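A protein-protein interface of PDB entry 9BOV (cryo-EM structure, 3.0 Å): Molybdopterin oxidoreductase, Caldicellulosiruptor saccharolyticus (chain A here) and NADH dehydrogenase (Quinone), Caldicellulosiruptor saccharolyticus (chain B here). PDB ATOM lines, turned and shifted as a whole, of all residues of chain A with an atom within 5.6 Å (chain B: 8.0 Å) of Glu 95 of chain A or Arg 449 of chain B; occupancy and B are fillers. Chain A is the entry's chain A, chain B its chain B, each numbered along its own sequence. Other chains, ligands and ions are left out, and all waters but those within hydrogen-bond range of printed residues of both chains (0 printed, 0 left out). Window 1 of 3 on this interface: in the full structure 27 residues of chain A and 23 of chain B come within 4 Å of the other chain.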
ATOM      1  N   GLU A  90      10.257 -21.986 -13.411  1.00  0.00           N
ATOM      2  CA  GLU A  90      11.030 -23.212 -13.587  1.00  0.00           C
ATOM      3  C   GLU A  90      11.857 -23.522 -12.347  1.00  0.00           C
ATOM      4  O   GLU A  90      11.944 -24.679 -11.918  1.00  0.00           O
ATOM      5  CB  GLU A  90      11.936 -23.092 -14.811  1.00  0.00           C
ATOM      6  CG  GLU A  90      11.220 -23.232 -16.139  1.00  0.00           C
ATOM      7  CD  GLU A  90      12.152 -23.053 -17.321  1.00  0.00           C
ATOM      8  OE1 GLU A  90      13.254 -22.497 -17.130  1.00  0.00           O
ATOM      9  OE2 GLU A  90      11.785 -23.462 -18.441  1.00  0.00           O
ATOM     10  N   LEU A  91      12.474 -22.497 -11.756  1.00  0.00           N
ATOM     11  CA  LEU A  91      13.258 -22.699 -10.545  1.00  0.00           C
ATOM     12  C   LEU A  91      12.381 -23.157  -9.387  1.00  0.00           C
ATOM     13  O   LEU A  91      12.783 -24.017  -8.597  1.00  0.00           O
ATOM     14  CB  LEU A  91      14.001 -21.414 -10.187  1.00  0.00           C
ATOM     15  CG  LEU A  91      15.249 -21.114 -11.014  1.00  0.00           C
ATOM     16  CD1 LEU A  91      15.980 -19.920 -10.448  1.00  0.00           C
ATOM     17  CD2 LEU A  91      16.161 -22.320 -11.055  1.00  0.00           C
ATOM     18  N   LEU A  92      11.181 -22.584  -9.263  1.00  0.00           N
ATOM     19  CA  LEU A  92      10.260 -23.020  -8.217  1.00  0.00           C
ATOM     20  C   LEU A  92       9.797 -24.454  -8.448  1.00  0.00           C
ATOM     21  O   LEU A  92       9.652 -25.225  -7.494  1.00  0.00           O
ATOM     22  CB  LEU A  92       9.062 -22.075  -8.144  1.00  0.00           C
ATOM     23  CG  LEU A  92       9.293 -20.751  -7.417  1.00  0.00           C
ATOM     24  CD1 LEU A  92       8.041 -19.901  -7.442  1.00  0.00           C
ATOM     25  CD2 LEU A  92       9.740 -20.999  -5.991  1.00  0.00           C
ATOM     26  N   LEU A  93       9.555 -24.825  -9.707  1.00  0.00           N
ATOM     27  CA  LEU A  93       9.122 -26.183 -10.019  1.00  0.00           C
ATOM     28  C   LEU A  93      10.229 -27.199  -9.786  1.00  0.00           C
ATOM     29  O   LEU A  93       9.943 -28.359  -9.471  1.00  0.00           O
ATOM     30  CB  LEU A  93       8.645 -26.263 -11.467  1.00  0.00           C
ATOM     31  CG  LEU A  93       7.241 -25.753 -11.777  1.00  0.00           C
ATOM     32  CD1 LEU A  93       6.914 -26.001 -13.235  1.00  0.00           C
ATOM     33  CD2 LEU A  93       6.217 -26.415 -10.875  1.00  0.00           C
ATOM     34  N   SER A  94      11.491 -26.794  -9.952  1.00  0.00           N
ATOM     35  CA  SER A  94      12.598 -27.734  -9.799  1.00  0.00           C
ATOM     36  C   SER A  94      12.636 -28.349  -8.406  1.00  0.00           C
ATOM     37  O   SER A  94      13.157 -29.455  -8.233  1.00  0.00           O
ATOM     38  CB  SER A  94      13.923 -27.040 -10.103  1.00  0.00           C
ATOM     39  OG  SER A  94      14.061 -25.851  -9.349  1.00  0.00           O
ATOM     40  N   GLU A  95      12.092 -27.656  -7.405  1.00  0.00           N
ATOM     41  CA  GLU A  95      12.059 -28.156  -6.036  1.00  0.00           C
ATOM     42  C   GLU A  95      10.645 -28.510  -5.585  1.00  0.00           C
ATOM     43  O   GLU A  95      10.373 -28.547  -4.382  1.00  0.00           O
ATOM     44  CB  GLU A  95      12.677 -27.132  -5.086  1.00  0.00           C
ATOM     45  CG  GLU A  95      12.219 -25.706  -5.326  1.00  0.00           C
ATOM     46  CD  GLU A  95      12.523 -24.793  -4.155  1.00  0.00           C
ATOM     47  OE1 GLU A  95      13.460 -25.099  -3.389  1.00  0.00           O
ATOM     48  OE2 GLU A  95      11.823 -23.770  -3.996  1.00  0.00           O
ATOM     49  N   HIS A  96       9.745 -28.778  -6.525  1.00  0.00           N
ATOM     50  CA  HIS A  96       8.349 -29.059  -6.226  1.00  0.00           C
ATOM     51  C   HIS A  96       8.081 -30.549  -6.376  1.00  0.00           C
ATOM     52  O   HIS A  96       8.390 -31.139  -7.417  1.00  0.00           O
ATOM     53  CB  HIS A  96       7.432 -28.263  -7.153  1.00  0.00           C
ATOM     54  CG  HIS A  96       6.059 -28.037  -6.605  1.00  0.00           C
ATOM     55  ND1 HIS A  96       5.766 -27.008  -5.736  1.00  0.00           N
ATOM     56  CD2 HIS A  96       4.896 -28.696  -6.812  1.00  0.00           C
ATOM     57  CE1 HIS A  96       4.483 -27.049  -5.427  1.00  0.00           C
ATOM     58  NE2 HIS A  96       3.932 -28.063  -6.068  1.00  0.00           N
ATOM     59  N   ARG A  97       7.502 -31.151  -5.340  1.00  0.00           N
ATOM     60  CA  ARG A  97       7.157 -32.571  -5.317  1.00  0.00           C
ATOM     61  C   ARG A  97       5.653 -32.673  -5.093  1.00  0.00           C
ATOM     62  O   ARG A  97       5.186 -32.708  -3.953  1.00  0.00           O
ATOM     63  CB  ARG A  97       7.931 -33.305  -4.234  1.00  0.00           C
ATOM     64  CG  ARG A  97       8.523 -34.625  -4.674  1.00  0.00           C
ATOM     65  CD  ARG A  97       9.122 -35.361  -3.495  1.00  0.00           C
ATOM     66  NE  ARG A  97      10.579 -35.342  -3.515  1.00  0.00           N
ATOM     67  CZ  ARG A  97      11.327 -36.182  -4.214  1.00  0.00           C
ATOM     68  NH1 ARG A  97      10.788 -37.119  -4.975  1.00  0.00           N
ATOM     69  NH2 ARG A  97      12.652 -36.082  -4.145  1.00  0.00           N
ATOM     70  N   TYR A 593      18.383 -32.123  -7.644  1.00  0.00           N
ATOM     71  CA  TYR A 593      18.078 -32.600  -6.303  1.00  0.00           C
ATOM     72  C   TYR A 593      16.786 -31.973  -5.802  1.00  0.00           C
ATOM     73  O   TYR A 593      16.568 -30.767  -5.944  1.00  0.00           O
ATOM     74  CB  TYR A 593      19.225 -32.279  -5.348  1.00  0.00           C
ATOM     75  CG  TYR A 593      18.958 -32.707  -3.923  1.00  0.00           C
ATOM     76  CD1 TYR A 593      18.762 -34.043  -3.606  1.00  0.00           C
ATOM     77  CD2 TYR A 593      18.898 -31.776  -2.897  1.00  0.00           C
ATOM     78  CE1 TYR A 593      18.516 -34.440  -2.307  1.00  0.00           C
ATOM     79  CE2 TYR A 593      18.653 -32.163  -1.595  1.00  0.00           C
ATOM     80  CZ  TYR A 593      18.462 -33.496  -1.306  1.00  0.00           C
ATOM     81  OH  TYR A 593      18.218 -33.888  -0.011  1.00  0.00           O
ATOM     82  N   LYS A 594      15.925 -32.800  -5.214  1.00  0.00           N
ATOM     83  CA  LYS A 594      14.635 -32.355  -4.709  1.00  0.00           C
ATOM     84  C   LYS A 594      14.414 -32.952  -3.330  1.00  0.00           C
ATOM     85  O   LYS A 594      14.576 -34.160  -3.143  1.00  0.00           O
ATOM     86  CB  LYS A 594      13.505 -32.764  -5.659  1.00  0.00           C
ATOM     87  CG  LYS A 594      12.177 -32.094  -5.374  1.00  0.00           C
ATOM     88  CD  LYS A 594      11.101 -32.562  -6.339  1.00  0.00           C
ATOM     89  CE  LYS A 594      11.651 -32.771  -7.735  1.00  0.00           C
ATOM     90  NZ  LYS A 594      10.600 -32.602  -8.771  1.00  0.00           N
ATOM     91  N   HIS A 595      14.045 -32.107  -2.373  1.00  0.00           N
ATOM     92  CA  HIS A 595      13.841 -32.565  -1.007  1.00  0.00           C
ATOM     93  C   HIS A 595      12.610 -33.456  -0.904  1.00  0.00           C
ATOM     94  O   HIS A 595      11.634 -33.299  -1.642  1.00  0.00           O
ATOM     95  CB  HIS A 595      13.693 -31.374  -0.062  1.00  0.00           C
ATOM     96  CG  HIS A 595      14.982 -30.684   0.254  1.00  0.00           C
ATOM     97  ND1 HIS A 595      16.001 -31.294   0.951  1.00  0.00           N
ATOM     98  CD2 HIS A 595      15.410 -29.430  -0.019  1.00  0.00           C
ATOM     99  CE1 HIS A 595      17.006 -30.448   1.087  1.00  0.00           C
ATOM    100  NE2 HIS A 595      16.673 -29.310   0.507  1.00  0.00           N
ATOM    101  N   ASP A 611       7.043 -30.390   0.894  1.00  0.00           N
ATOM    102  CA  ASP A 611       7.471 -30.661  -0.474  1.00  0.00           C
ATOM    103  C   ASP A 611       6.826 -29.729  -1.489  1.00  0.00           C
ATOM    104  O   ASP A 611       7.339 -29.603  -2.605  1.00  0.00           O
ATOM    105  CB  ASP A 611       7.165 -32.112  -0.834  1.00  0.00           C
ATOM    106  CG  ASP A 611       7.969 -33.093  -0.014  1.00  0.00           C
ATOM    107  OD1 ASP A 611       9.048 -32.709   0.482  1.00  0.00           O
ATOM    108  OD2 ASP A 611       7.526 -34.250   0.135  1.00  0.00           O
ATOM    109  N   CYS A 613       6.158 -26.419  -0.716  1.00  0.00           N
ATOM    110  CA  CYS A 613       6.368 -25.077  -0.196  1.00  0.00           C
ATOM    111  C   CYS A 613       7.302 -24.307  -1.119  1.00  0.00           C
ATOM    112  O   CYS A 613       8.413 -24.761  -1.406  1.00  0.00           O
ATOM    113  CB  CYS A 613       6.947 -25.136   1.215  1.00  0.00           C
ATOM    114  SG  CYS A 613       7.321 -23.534   1.940  1.00  0.00           S
ATOM    115  N   ILE A 614       6.846 -23.144  -1.583  1.00  0.00           N
ATOM    116  CA  ILE A 614       7.667 -22.262  -2.399  1.00  0.00           C
ATOM    117  C   ILE A 614       8.362 -21.201  -1.556  1.00  0.00           C
ATOM    118  O   ILE A 614       8.960 -20.273  -2.104  1.00  0.00           O
ATOM    119  CB  ILE A 614       6.844 -21.618  -3.524  1.00  0.00           C
ATOM    120  CG1 ILE A 614       5.754 -20.720  -2.946  1.00  0.00           C
ATOM    121  CG2 ILE A 614       6.234 -22.686  -4.409  1.00  0.00           C
ATOM    122  CD1 ILE A 614       5.196 -19.730  -3.934  1.00  0.00           C
ATOM    123  N   LEU A 615       8.292 -21.323  -0.230  1.00  0.00           N
ATOM    124  CA  LEU A 615       9.018 -20.460   0.700  1.00  0.00           C
ATOM    125  C   LEU A 615       8.734 -18.984   0.445  1.00  0.00           C
ATOM    126  O   LEU A 615       9.634 -18.143   0.457  1.00  0.00           O
ATOM    127  CB  LEU A 615      10.516 -20.748   0.650  1.00  0.00           C
ATOM    128  CG  LEU A 615      10.942 -21.980   1.449  1.00  0.00           C
ATOM    129  CD1 LEU A 615      12.337 -22.417   1.069  1.00  0.00           C
ATOM    130  CD2 LEU A 615      10.864 -21.691   2.927  1.00  0.00           C
ATOM    131  N   GLY A 638      19.359 -21.358   3.408  1.00  0.00           N
ATOM    132  CA  GLY A 638      19.758 -21.699   2.059  1.00  0.00           C
ATOM    133  C   GLY A 638      18.802 -22.651   1.375  1.00  0.00           C
ATOM    134  O   GLY A 638      17.582 -22.506   1.485  1.00  0.00           O
ATOM    135  N   PHE A 639      19.352 -23.631   0.657  1.00  0.00           N
ATOM    136  CA  PHE A 639      18.521 -24.632   0.001  1.00  0.00           C
ATOM    137  C   PHE A 639      17.768 -25.498   1.001  1.00  0.00           C
ATOM    138  O   PHE A 639      16.761 -26.112   0.635  1.00  0.00           O
ATOM    139  CB  PHE A 639      19.384 -25.509  -0.903  1.00  0.00           C
ATOM    140  CG  PHE A 639      18.602 -26.309  -1.900  1.00  0.00           C
ATOM    141  CD1 PHE A 639      18.004 -25.695  -2.985  1.00  0.00           C
ATOM    142  CD2 PHE A 639      18.470 -27.677  -1.759  1.00  0.00           C
ATOM    143  CE1 PHE A 639      17.285 -26.429  -3.902  1.00  0.00           C
ATOM    144  CE2 PHE A 639      17.752 -28.416  -2.674  1.00  0.00           C
ATOM    145  CZ  PHE A 639      17.159 -27.791  -3.746  1.00  0.00           C
ATOM    146  N   THR A 641      16.222 -24.469   3.756  1.00  0.00           N
ATOM    147  CA  THR A 641      15.238 -23.730   4.533  1.00  0.00           C
ATOM    148  C   THR A 641      13.896 -24.448   4.520  1.00  0.00           C
ATOM    149  O   THR A 641      13.485 -25.012   3.503  1.00  0.00           O
ATOM    150  CB  THR A 641      15.075 -22.314   3.980  1.00  0.00           C
ATOM    151  OG1 THR A 641      16.339 -21.841   3.504  1.00  0.00           O
ATOM    152  CG2 THR A 641      14.574 -21.381   5.058  1.00  0.00           C
ATOM    153  N   THR B 437      29.066 -20.205  -2.244  1.00  0.00           N
ATOM    154  CA  THR B 437      27.990 -19.218  -2.271  1.00  0.00           C
ATOM    155  C   THR B 437      26.624 -19.877  -2.107  1.00  0.00           C
ATOM    156  O   THR B 437      25.752 -19.344  -1.410  1.00  0.00           O
ATOM    157  CB  THR B 437      28.049 -18.406  -3.561  1.00  0.00           C
ATOM    158  OG1 THR B 437      29.298 -17.707  -3.623  1.00  0.00           O
ATOM    159  CG2 THR B 437      26.928 -17.393  -3.590  1.00  0.00           C
ATOM    160  N   CYS B 438      26.418 -21.040  -2.731  1.00  0.00           N
ATOM    161  CA  CYS B 438      25.164 -21.764  -2.558  1.00  0.00           C
ATOM    162  C   CYS B 438      24.967 -22.179  -1.108  1.00  0.00           C
ATOM    163  O   CYS B 438      23.847 -22.130  -0.587  1.00  0.00           O
ATOM    164  CB  CYS B 438      25.130 -22.985  -3.473  1.00  0.00           C
ATOM    165  SG  CYS B 438      24.014 -24.292  -2.922  1.00  0.00           S
ATOM    166  N   LYS B 439      26.041 -22.599  -0.439  1.00  0.00           N
ATOM    167  CA  LYS B 439      25.932 -22.923   0.979  1.00  0.00           C
ATOM    168  C   LYS B 439      25.653 -21.686   1.821  1.00  0.00           C
ATOM    169  O   LYS B 439      25.011 -21.789   2.872  1.00  0.00           O
ATOM    170  CB  LYS B 439      27.204 -23.619   1.463  1.00  0.00           C
ATOM    171  CG  LYS B 439      27.396 -25.018   0.906  1.00  0.00           C
ATOM    172  CD  LYS B 439      26.849 -26.067   1.860  1.00  0.00           C
ATOM    173  CE  LYS B 439      26.811 -27.442   1.214  1.00  0.00           C
ATOM    174  NZ  LYS B 439      25.693 -27.571   0.242  1.00  0.00           N
ATOM    175  N   SER B 441      23.907 -18.932   0.913  1.00  0.00           N
ATOM    176  CA  SER B 441      22.666 -18.226   0.630  1.00  0.00           C
ATOM    177  C   SER B 441      21.706 -18.350   1.807  1.00  0.00           C
ATOM    178  O   SER B 441      21.749 -19.318   2.569  1.00  0.00           O
ATOM    179  CB  SER B 441      22.011 -18.780  -0.631  1.00  0.00           C
ATOM    180  OG  SER B 441      21.170 -19.875  -0.322  1.00  0.00           O
ATOM    181  N   CYS B 442      20.836 -17.351   1.958  1.00  0.00           N
ATOM    182  CA  CYS B 442      19.857 -17.363   3.037  1.00  0.00           C
ATOM    183  C   CYS B 442      18.558 -18.061   2.657  1.00  0.00           C
ATOM    184  O   CYS B 442      17.828 -18.508   3.549  1.00  0.00           O
ATOM    185  CB  CYS B 442      19.550 -15.935   3.497  1.00  0.00           C
ATOM    186  SG  CYS B 442      18.235 -15.117   2.586  1.00  0.00           S
ATOM    187  N   GLY B 443      18.251 -18.163   1.366  1.00  0.00           N
ATOM    188  CA  GLY B 443      17.119 -18.947   0.915  1.00  0.00           C
ATOM    189  C   GLY B 443      15.812 -18.206   0.754  1.00  0.00           C
ATOM    190  O   GLY B 443      14.767 -18.851   0.634  1.00  0.00           O
ATOM    191  N   LYS B 444      15.827 -16.875   0.745  1.00  0.00           N
ATOM    192  CA  LYS B 444      14.575 -16.135   0.650  1.00  0.00           C
ATOM    193  C   LYS B 444      14.001 -16.186  -0.763  1.00  0.00           C
ATOM    194  O   LYS B 444      12.874 -16.647  -0.968  1.00  0.00           O
ATOM    195  CB  LYS B 444      14.782 -14.686   1.096  1.00  0.00           C
ATOM    196  CG  LYS B 444      13.644 -13.760   0.711  1.00  0.00           C
ATOM    197  CD  LYS B 444      14.065 -12.307   0.779  1.00  0.00           C
ATOM    198  CE  LYS B 444      13.830 -11.735   2.161  1.00  0.00           C
ATOM    199  NZ  LYS B 444      13.738 -10.252   2.131  1.00  0.00           N
ATOM    200  N   CYS B 445      14.763 -15.724  -1.751  1.00  0.00           N
ATOM    201  CA  CYS B 445      14.259 -15.623  -3.114  1.00  0.00           C
ATOM    202  C   CYS B 445      14.622 -16.859  -3.924  1.00  0.00           C
ATOM    203  O   CYS B 445      15.656 -17.493  -3.701  1.00  0.00           O
ATOM    204  CB  CYS B 445      14.797 -14.370  -3.806  1.00  0.00           C
ATOM    205  SG  CYS B 445      16.580 -14.192  -3.779  1.00  0.00           S
ATOM    206  N   THR B 446      13.752 -17.191  -4.880  1.00  0.00           N
ATOM    207  CA  THR B 446      13.906 -18.431  -5.634  1.00  0.00           C
ATOM    208  C   THR B 446      15.186 -18.438  -6.461  1.00  0.00           C
ATOM    209  O   THR B 446      15.867 -19.465  -6.546  1.00  0.00           O
ATOM    210  CB  THR B 446      12.690 -18.655  -6.534  1.00  0.00           C
ATOM    211  OG1 THR B 446      12.967 -19.709  -7.463  1.00  0.00           O
ATOM    212  CG2 THR B 446      12.346 -17.394  -7.298  1.00  0.00           C
ATOM    213  N   TYR B 447      15.532 -17.305  -7.074  1.00  0.00           N
ATOM    214  CA  TYR B 447      16.657 -17.283  -8.002  1.00  0.00           C
ATOM    215  C   TYR B 447      17.961 -17.662  -7.314  1.00  0.00           C
ATOM    216  O   TYR B 447      18.770 -18.409  -7.876  1.00  0.00           O
ATOM    217  CB  TYR B 447      16.775 -15.909  -8.647  1.00  0.00           C
ATOM    218  CG  TYR B 447      15.733 -15.632  -9.699  1.00  0.00           C
ATOM    219  CD1 TYR B 447      15.630 -16.431 -10.827  1.00  0.00           C
ATOM    220  CD2 TYR B 447      14.858 -14.564  -9.570  1.00  0.00           C
ATOM    221  CE1 TYR B 447      14.683 -16.176 -11.795  1.00  0.00           C
ATOM    222  CE2 TYR B 447      13.910 -14.301 -10.533  1.00  0.00           C
ATOM    223  CZ  TYR B 447      13.825 -15.109 -11.643  1.00  0.00           C
ATOM    224  OH  TYR B 447      12.879 -14.849 -12.604  1.00  0.00           O
ATOM    225  N   CYS B 448      18.193 -17.155  -6.105  1.00  0.00           N
ATOM    226  CA  CYS B 448      19.436 -17.480  -5.416  1.00  0.00           C
ATOM    227  C   CYS B 448      19.351 -18.797  -4.657  1.00  0.00           C
ATOM    228  O   CYS B 448      20.346 -19.524  -4.580  1.00  0.00           O
ATOM    229  CB  CYS B 448      19.824 -16.356  -4.457  1.00  0.00           C
ATOM    230  SG  CYS B 448      21.188 -16.771  -3.346  1.00  0.00           S
ATOM    231  N   ARG B 449      18.187 -19.122  -4.092  1.00  0.00           N
ATOM    232  CA  ARG B 449      18.093 -20.298  -3.234  1.00  0.00           C
ATOM    233  C   ARG B 449      18.224 -21.585  -4.035  1.00  0.00           C
ATOM    234  O   ARG B 449      18.998 -22.479  -3.670  1.00  0.00           O
ATOM    235  CB  ARG B 449      16.777 -20.285  -2.461  1.00  0.00           C
ATOM    236  CG  ARG B 449      16.584 -21.492  -1.564  1.00  0.00           C
ATOM    237  CD  ARG B 449      15.154 -21.589  -1.075  1.00  0.00           C
ATOM    238  NE  ARG B 449      14.217 -21.835  -2.163  1.00  0.00           N
ATOM    239  CZ  ARG B 449      13.159 -21.080  -2.421  1.00  0.00           C
ATOM    240  NH1 ARG B 449      12.874 -20.018  -1.688  1.00  0.00           N
ATOM    241  NH2 ARG B 449      12.369 -21.398  -3.442  1.00  0.00           N
ATOM    242  N   VAL B 450      17.475 -21.703  -5.129  1.00  0.00           N
ATOM    243  CA  VAL B 450      17.468 -22.923  -5.914  1.00  0.00           C
ATOM    244  C   VAL B 450      18.227 -22.780  -7.230  1.00  0.00           C
ATOM    245  O   VAL B 450      18.748 -23.779  -7.738  1.00  0.00           O
ATOM    246  CB  VAL B 450      16.020 -23.402  -6.161  1.00  0.00           C
ATOM    247  CG1 VAL B 450      15.287 -22.454  -7.078  1.00  0.00           C
ATOM    248  CG2 VAL B 450      15.998 -24.810  -6.721  1.00  0.00           C
ATOM    249  N   GLY B 451      18.334 -21.570  -7.782  1.00  0.00           N
ATOM    250  CA  GLY B 451      19.094 -21.393  -9.008  1.00  0.00           C
ATOM    251  C   GLY B 451      20.565 -21.713  -8.834  1.00  0.00           C
ATOM    252  O   GLY B 451      21.181 -22.350  -9.695  1.00  0.00           O
ATOM    253  N   THR B 452      21.148 -21.286  -7.712  1.00  0.00           N
ATOM    254  CA  THR B 452      22.550 -21.588  -7.448  1.00  0.00           C
ATOM    255  C   THR B 452      22.777 -23.088  -7.337  1.00  0.00           C
ATOM    256  O   THR B 452      23.806 -23.604  -7.785  1.00  0.00           O
ATOM    257  CB  THR B 452      23.017 -20.879  -6.175  1.00  0.00           C
ATOM    258  OG1 THR B 452      22.061 -21.086  -5.130  1.00  0.00           O
ATOM    259  CG2 THR B 452      23.173 -19.390  -6.429  1.00  0.00           C
ATOM    260  N   ARG B 453      21.826 -23.808  -6.747  1.00  0.00           N
ATOM    261  CA  ARG B 453      21.956 -25.257  -6.669  1.00  0.00           C
ATOM    262  C   ARG B 453      21.902 -25.889  -8.050  1.00  0.00           C
ATOM    263  O   ARG B 453      22.675 -26.806  -8.352  1.00  0.00           O
ATOM    264  CB  ARG B 453      20.871 -25.832  -5.769  1.00  0.00           C
ATOM    265  CG  ARG B 453      21.079 -27.283  -5.417  1.00  0.00           C
ATOM    266  CD  ARG B 453      22.344 -27.459  -4.603  1.00  0.00           C
ATOM    267  NE  ARG B 453      22.095 -28.165  -3.353  1.00  0.00           N
ATOM    268  CZ  ARG B 453      22.929 -28.180  -2.323  1.00  0.00           C
ATOM    269  NH1 ARG B 453      24.087 -27.542  -2.361  1.00  0.00           N
ATOM    270  NH2 ARG B 453      22.590 -28.850  -1.225  1.00  0.00           N
ATOM    271  N   ARG B 454      20.994 -25.420  -8.907  1.00  0.00           N
ATOM    272  CA  ARG B 454      20.930 -25.973 -10.254  1.00  0.00           C
ATOM    273  C   ARG B 454      22.227 -25.711 -11.006  1.00  0.00           C
ATOM    274  O   ARG B 454      22.722 -26.587 -11.725  1.00  0.00           O
ATOM    275  CB  ARG B 454      19.731 -25.400 -11.009  1.00  0.00           C
ATOM    276  CG  ARG B 454      18.409 -25.571 -10.283  1.00  0.00           C
ATOM    277  CD  ARG B 454      18.246 -27.000  -9.769  1.00  0.00           C
ATOM    278  NE  ARG B 454      17.307 -27.090  -8.655  1.00  0.00           N
ATOM    279  CZ  ARG B 454      17.218 -28.119  -7.823  1.00  0.00           C
ATOM    280  NH1 ARG B 454      18.012 -29.168  -7.936  1.00  0.00           N
ATOM    281  NH2 ARG B 454      16.318 -28.089  -6.844  1.00  0.00           N
ATOM    282  N   VAL B 482      19.857 -15.795 -12.737  1.00  0.00           N
ATOM    283  CA  VAL B 482      20.094 -15.654 -11.305  1.00  0.00           C
ATOM    284  C   VAL B 482      20.699 -14.291 -10.999  1.00  0.00           C
ATOM    285  O   VAL B 482      20.349 -13.649 -10.003  1.00  0.00           O
ATOM    286  CB  VAL B 482      20.988 -16.799 -10.801  1.00  0.00           C
ATOM    287  CG1 VAL B 482      21.478 -16.520  -9.396  1.00  0.00           C
ATOM    288  CG2 VAL B 482      20.239 -18.109 -10.851  1.00  0.00           C
ATOM    289  N   SER B 486      17.990 -12.168  -8.705  1.00  0.00           N
ATOM    290  CA  SER B 486      18.156 -12.336  -7.272  1.00  0.00           C
ATOM    291  C   SER B 486      17.912 -11.019  -6.544  1.00  0.00           C
ATOM    292  O   SER B 486      18.040  -9.931  -7.109  1.00  0.00           O
ATOM    293  CB  SER B 486      19.553 -12.864  -6.951  1.00  0.00           C
ATOM    294  OG  SER B 486      19.815 -14.064  -7.652  1.00  0.00           O
ATOM    295  N   GLY B 491      23.242 -13.019  -4.341  1.00  0.00           N
ATOM    296  CA  GLY B 491      22.732 -13.755  -5.477  1.00  0.00           C
ATOM    297  C   GLY B 491      23.080 -13.080  -6.784  1.00  0.00           C
ATOM    298  O   GLY B 491      23.338 -13.750  -7.787  1.00  0.00           O
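Glu 95 of chain A touches just one residue of chain B: Arg 449 (2.5 Å). Arg 449 of chain B touches six residues of chain A. Of chain B, only Val 450 (3.4 Å) and Arg 454 (3.5 Å) come within 4 Å of Ser 94 of chain A. Printed residues of chain A within 4 Å of Cys 442 of chain B: Gly 638 and Thr 641. Printed residues of chain A within 4 Å of Ser 441 of chain B: Gly 638 (3.1 Å). Thr 437 of chain B touches none of the printed residues of chain A. Leu 93 of chain A touches none of the printed residues of chain B. The nearest printed residue of chain B that does not touch Glu 95 of chain A is Val 450 of chain B (4.1 Å). The nearest printed residue of chain A that does not touch Tyr 447 of chain B is Leu 92 of chain A (7.0 Å).
Printed residues of chain B that touch a printed residue of chain A: Ser 441, Cys 442, Gly 443, Lys 444, Thr 446, Tyr 447, Arg 449, Val 450, Gly 451, Arg 453 and Arg 454. Hydrophobic or aromatic side chains of chain B that line the printed part of chain A: Tyr 447 and Val 450. Along chain B the printed residues that touch a printed residue of chain A span positions 441 to 454. Hydrophobic or aromatic side chains of chain A within 4 Å of the printed part of chain B: Leu 91, Leu 92, Leu 615 and Phe 639. Among the printed residues, Asp or Glu carboxylates within 4 Å of a Lys or Arg side-chain nitrogen of the other chain: Glu 95 of chain A with Arg 449 of chain B.
Leu 91 of chain A touches Thr 446 of chain B. Leu 91 of chain A touches Tyr 447 of chain B. Leu 91 of chain A touches Gly 451 of chain B (CD2 to CA, 3.7 Å). Thr 446 of chain B touches Leu 92 of chain A. OG of Ser 94 of chain A touches CG2 of Val 450 of chain B, 3.4 Å away. Ile 614 of chain A touches Arg 449 of chain B (O to NH2, 3.8 Å). Leu 615 of chain A touches Lys 444 of chain B (O to O, 3.8 Å). Arg 449 of chain B touches Phe 639 of chain A. Phe 639 of chain A touches Arg 453 of chain B. Gly 443 of chain B touches Thr 641 of chain A (CA to OG1, 3.96 Å).
The guanidinium group (NH2) of Arg 449 of chain B lies within salt-bridge range of the side-chain carboxylate (OE2) of Glu 95 of chain A, at 2.5 Å. The backbone carbonyl oxygen (O) of Tyr 593 of chain A lies within hydrogen-bond range of the guanidinium group (NH2) of Arg 454 of chain B (2.8 Å). The backbone carbonyl oxygen of Ser 441 of chain B sits close to the backbone NH of Gly 638 of chain A, 3.3 Å away. The backbone carbonyl oxygen (O) of Cys 442 of chain B is in hydrogen-bond range of the backbone NH (N) of Gly 638 of chain A.
A ring nitrogen (NE2) of His 595 of chain A lies within hydrogen-bond range of the backbone carbonyl oxygen of Phe 639 of chain A. The side-chain sulfur of Cys 613 of chain A lies close to the backbone NH of Leu 615 of chain A, at 3.2 Å. The side-chain sulfur (SG) of Cys 442 of chain B sits close to the backbone NH (N) of Lys 444 of chain B (3.5 Å). O of Gly 443 of chain B sits at hydrogen-bond distance from NH1 of Arg 449 of chain B, 3.2 Å away. The guanidinium group of Arg 449 of chain B sits at hydrogen-bond distance from the backbone carbonyl oxygen of Lys 444 of chain B (3.4 Å). The backbone carbonyl oxygen of Thr 446 of chain B lies within hydrogen-bond range of the backbone NH of Gly 451 of chain B, 3.5 Å away.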
